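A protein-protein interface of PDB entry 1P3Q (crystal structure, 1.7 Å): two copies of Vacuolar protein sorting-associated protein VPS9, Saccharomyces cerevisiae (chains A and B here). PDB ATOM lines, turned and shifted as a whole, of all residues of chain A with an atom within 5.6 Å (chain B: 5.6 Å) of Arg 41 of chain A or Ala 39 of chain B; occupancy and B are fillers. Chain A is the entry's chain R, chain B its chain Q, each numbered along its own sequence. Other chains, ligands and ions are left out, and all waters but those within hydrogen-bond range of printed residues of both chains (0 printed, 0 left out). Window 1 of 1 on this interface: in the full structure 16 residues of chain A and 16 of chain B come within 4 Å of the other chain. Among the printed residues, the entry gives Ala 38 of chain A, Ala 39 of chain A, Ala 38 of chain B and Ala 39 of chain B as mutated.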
ATOM      1  N   ALA A  37      11.761  32.211  30.248  1.00  0.00           N
ATOM      2  CA  ALA A  37      13.083  32.306  29.553  1.00  0.00           C
ATOM      3  C   ALA A  37      13.445  30.945  28.994  1.00  0.00           C
ATOM      4  O   ALA A  37      14.149  30.800  27.996  1.00  0.00           O
ATOM      5  CB  ALA A  37      14.157  32.817  30.494  1.00  0.00           C
ATOM      6  N   ALA A  38      12.899  30.019  29.754  1.00  0.00           N
ATOM      7  CA  ALA A  38      13.093  28.627  29.373  1.00  0.00           C
ATOM      8  C   ALA A  38      12.025  28.308  28.334  1.00  0.00           C
ATOM      9  O   ALA A  38      12.297  27.671  27.312  1.00  0.00           O
ATOM     10  CB  ALA A  38      12.936  27.726  30.590  1.00  0.00           C
ATOM     11  N   ALA A  39      10.810  28.773  28.614  1.00  0.00           N
ATOM     12  CA  ALA A  39       9.658  28.578  27.738  1.00  0.00           C
ATOM     13  C   ALA A  39       9.659  29.723  26.740  1.00  0.00           C
ATOM     14  O   ALA A  39       8.698  30.492  26.629  1.00  0.00           O
ATOM     15  CB  ALA A  39       8.361  28.582  28.560  1.00  0.00           C
ATOM     16  N   SER A  40      10.774  29.818  26.029  1.00  0.00           N
ATOM     17  CA  SER A  40      11.031  30.834  25.022  1.00  0.00           C
ATOM     18  C   SER A  40      12.374  30.439  24.450  1.00  0.00           C
ATOM     19  O   SER A  40      12.683  30.688  23.289  1.00  0.00           O
ATOM     20  CB  SER A  40      11.146  32.214  25.673  1.00  0.00           C
ATOM     21  OG  SER A  40      12.081  33.028  24.980  1.00  0.00           O
ATOM     22  N   ARG A  41      13.165  29.798  25.298  1.00  0.00           N
ATOM     23  CA  ARG A  41      14.488  29.359  24.927  1.00  0.00           C
ATOM     24  C   ARG A  41      15.192  30.510  24.217  1.00  0.00           C
ATOM     25  O   ARG A  41      15.696  30.355  23.109  1.00  0.00           O
ATOM     26  CB  ARG A  41      14.405  28.121  24.022  1.00  0.00           C
ATOM     27  CG  ARG A  41      15.493  27.084  24.319  1.00  0.00           C
ATOM     28  CD  ARG A  41      15.510  26.695  25.813  1.00  0.00           C
ATOM     29  NE  ARG A  41      16.711  25.944  26.201  1.00  0.00           N
ATOM     30  CZ  ARG A  41      16.939  25.477  27.428  1.00  0.00           C
ATOM     31  NH1 ARG A  41      16.047  25.675  28.388  1.00  0.00           N
ATOM     32  NH2 ARG A  41      18.063  24.825  27.703  1.00  0.00           N
ATOM     33  N   ILE A  42      15.190  31.676  24.858  1.00  0.00           N
ATOM     34  CA  ILE A  42      15.850  32.841  24.294  1.00  0.00           C
ATOM     35  C   ILE A  42      17.341  32.599  24.490  1.00  0.00           C
ATOM     36  O   ILE A  42      18.175  33.127  23.748  1.00  0.00           O
ATOM     37  CB  ILE A  42      15.434  34.158  25.009  1.00  0.00           C
ATOM     38  CG1 ILE A  42      16.116  35.354  24.336  1.00  0.00           C
ATOM     39  CG2 ILE A  42      15.805  34.101  26.493  1.00  0.00           C
ATOM     40  CD1 ILE A  42      16.149  36.592  25.202  1.00  0.00           C
ATOM     41  N   GLY A  43      17.667  31.785  25.495  1.00  0.00           N
ATOM     42  CA  GLY A  43      19.056  31.452  25.766  1.00  0.00           C
ATOM     43  C   GLY A  43      19.725  30.764  24.586  1.00  0.00           C
ATOM     44  O   GLY A  43      20.760  31.215  24.119  1.00  0.00           O
ATOM     45  N   PRO A  44      19.173  29.643  24.099  1.00  0.00           N
ATOM     46  CA  PRO A  44      19.788  28.954  22.952  1.00  0.00           C
ATOM     47  C   PRO A  44      19.742  29.777  21.665  1.00  0.00           C
ATOM     48  O   PRO A  44      20.624  29.659  20.809  1.00  0.00           O
ATOM     49  CB  PRO A  44      18.977  27.666  22.851  1.00  0.00           C
ATOM     50  CG  PRO A  44      18.680  27.369  24.298  1.00  0.00           C
ATOM     51  CD  PRO A  44      18.245  28.749  24.807  1.00  0.00           C
ATOM     52  N   CYS A  45      18.704  30.595  21.516  1.00  0.00           N
ATOM     53  CA  CYS A  45      18.604  31.446  20.336  1.00  0.00           C
ATOM     54  C   CYS A  45      19.784  32.391  20.360  1.00  0.00           C
ATOM     55  O   CYS A  45      20.354  32.694  19.323  1.00  0.00           O
ATOM     56  CB  CYS A  45      17.314  32.270  20.323  1.00  0.00           C
ATOM     57  SG  CYS A  45      15.828  31.369  19.972  1.00  0.00           S
ATOM     58  N   VAL A  46      20.141  32.871  21.553  1.00  0.00           N
ATOM     59  CA  VAL A  46      21.273  33.778  21.701  1.00  0.00           C
ATOM     60  C   VAL A  46      22.557  32.993  21.461  1.00  0.00           C
ATOM     61  O   VAL A  46      23.531  33.542  20.940  1.00  0.00           O
ATOM     62  CB  VAL A  46      21.299  34.453  23.131  1.00  0.00           C
ATOM     63  CG1 VAL A  46      22.626  35.171  23.362  1.00  0.00           C
ATOM     64  CG2 VAL A  46      20.158  35.477  23.238  1.00  0.00           C
ATOM     65  N   THR B  15       9.950  36.543  21.179  1.00  0.00           N
ATOM     66  CA  THR B  15      11.380  36.264  21.163  1.00  0.00           C
ATOM     67  C   THR B  15      12.067  36.957  19.994  1.00  0.00           C
ATOM     68  O   THR B  15      13.170  37.488  20.142  1.00  0.00           O
ATOM     69  CB  THR B  15      11.642  34.746  21.095  1.00  0.00           C
ATOM     70  OG1 THR B  15      11.175  34.135  22.306  1.00  0.00           O
ATOM     71  CG2 THR B  15      13.130  34.457  20.940  1.00  0.00           C
ATOM     72  N   CYS B  35      15.676  31.369  15.102  1.00  0.00           N
ATOM     73  CA  CYS B  35      14.698  31.218  16.176  1.00  0.00           C
ATOM     74  C   CYS B  35      13.882  29.954  15.941  1.00  0.00           C
ATOM     75  O   CYS B  35      13.731  29.124  16.837  1.00  0.00           O
ATOM     76  CB  CYS B  35      13.783  32.439  16.222  1.00  0.00           C
ATOM     77  N   ALA B  37      14.646  27.259  14.314  1.00  0.00           N
ATOM     78  CA  ALA B  37      15.448  26.067  14.564  1.00  0.00           C
ATOM     79  C   ALA B  37      15.904  25.953  16.031  1.00  0.00           C
ATOM     80  O   ALA B  37      16.279  24.863  16.493  1.00  0.00           O
ATOM     81  CB  ALA B  37      16.657  26.058  13.660  1.00  0.00           C
ATOM     82  N   ALA B  38      15.870  27.079  16.743  1.00  0.00           N
ATOM     83  CA  ALA B  38      16.297  27.151  18.146  1.00  0.00           C
ATOM     84  C   ALA B  38      15.479  26.346  19.159  1.00  0.00           C
ATOM     85  O   ALA B  38      14.257  26.260  19.066  1.00  0.00           O
ATOM     86  CB  ALA B  38      16.351  28.602  18.583  1.00  0.00           C
ATOM     87  N   ALA B  39      16.190  25.788  20.141  1.00  0.00           N
ATOM     88  CA  ALA B  39      15.627  24.959  21.207  1.00  0.00           C
ATOM     89  C   ALA B  39      14.328  25.433  21.857  1.00  0.00           C
ATOM     90  O   ALA B  39      13.778  26.479  21.513  1.00  0.00           O
ATOM     91  CB  ALA B  39      16.688  24.735  22.294  1.00  0.00           C
ATOM     92  N   SER B  40      13.865  24.632  22.814  1.00  0.00           N
ATOM     93  CA  SER B  40      12.641  24.869  23.577  1.00  0.00           C
ATOM     94  C   SER B  40      12.014  26.245  23.363  1.00  0.00           C
ATOM     95  O   SER B  40      11.069  26.396  22.589  1.00  0.00           O
ATOM     96  CB  SER B  40      12.922  24.665  25.069  1.00  0.00           C
ATOM     97  OG  SER B  40      13.630  23.456  25.296  1.00  0.00           O
ATOM     98  N   PRO B  44      12.781  22.927  32.348  1.00  0.00           N
ATOM     99  CA  PRO B  44      13.835  23.947  32.297  1.00  0.00           C
ATOM    100  C   PRO B  44      13.604  25.014  33.372  1.00  0.00           C
ATOM    101  O   PRO B  44      14.533  25.403  34.083  1.00  0.00           O
ATOM    102  CB  PRO B  44      13.701  24.494  30.882  1.00  0.00           C
ATOM    103  CG  PRO B  44      13.331  23.261  30.106  1.00  0.00           C
ATOM    104  CD  PRO B  44      12.276  22.634  30.993  1.00  0.00           C
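Printed residues of chain B that touch a printed residue of chain A: Thr 15, Cys 35, Ala 38, Ala 39, Ser 40 and Pro 44.
Of the 10 printed residues of chain A, 5 touch a printed residue of chain B.
Printed residues of chain A that touch a printed residue of chain B: Ala 38, Ser 40, Arg 41, Pro 44 and Cys 45.
Among the printed residues, 9 pairs touch across the chains.
OG of Ser 40 of chain A is in hydrogen-bond range of OG1 of Thr 15 of chain B (3.0 Å).
Ala 37 of chain A touches none of the printed residues of chain B.
Of the printed residues of chain B, Ala 38 of chain A touches Ser 40 and Pro 44.
Ala 39 of chain A touches none of the printed residues of chain B.
Of the printed residues of chain B, Ser 40 of chain A touches Thr 15.
Arg 41 of chain A touches just these residues of chain B: Ala 39, Ser 40 and Pro 44.
Of the printed residues of chain B, Cys 45 of chain A touches Cys 35 and Ala 38.
Printed residues of chain A within 4 Å of Ser 40 of chain B: Ala 38 and Arg 41.
The nearest residue of chain A that does not touch Ala 39 of chain B is Ser 40 of chain A (4.7 Å).
The nearest printed residue of chain B that does not touch Cys 45 of chain A is Thr 15 of chain B (4.2 Å).
Among the printed residues, pairs that only touch across the chains: Ala 38 of chain A with Ser 40 of chain B (3.8 Å), Ala 38 of chain A with Pro 44 of chain B (3.3 Å), Arg 41 of chain A with Ala 39 of chain B (3.1 Å), Arg 41 of chain A with Ser 40 of chain B (3.1 Å), Arg 41 of chain A with Pro 44 of chain B (3.6 Å), Pro 44 of chain A with Ala 39 of chain B (3.8 Å), Cys 45 of chain A with Cys 35 of chain B (3.96 Å) and Cys 45 of chain A with Ala 38 of chain B (3.1 Å).
The side-chain hydroxyl (OG) of Ser 40 of chain A lies close to the backbone NH (N) of Ile 42 of chain A (3.4 Å).
O of Arg 41 of chain A sits at hydrogen-bond distance from SG of Cys 45 of chain A (3.3 Å).
Ala 38 of chain A touches Ser 40 of chain B, but with the chains exchanged Ser 40 of chain A does not touch Ala 38 of chain B (6.3 Å).
Ala 38 of chain A touches Pro 44 of chain B, but with the chains exchanged Pro 44 of chain A does not touch Ala 38 of chain B (4.7 Å).
Pro 44 of chain A touches Ala 39 of chain B, but with the chains exchanged Ala 39 of chain A does not touch Pro 44 of chain B (5.6 Å).
Positions printed for both chains: 37, 38, 39, 40 and 44.
Of the 9 pairs that touch across the chains among the printed residues, none has its exchanged pair printed and touching as well.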
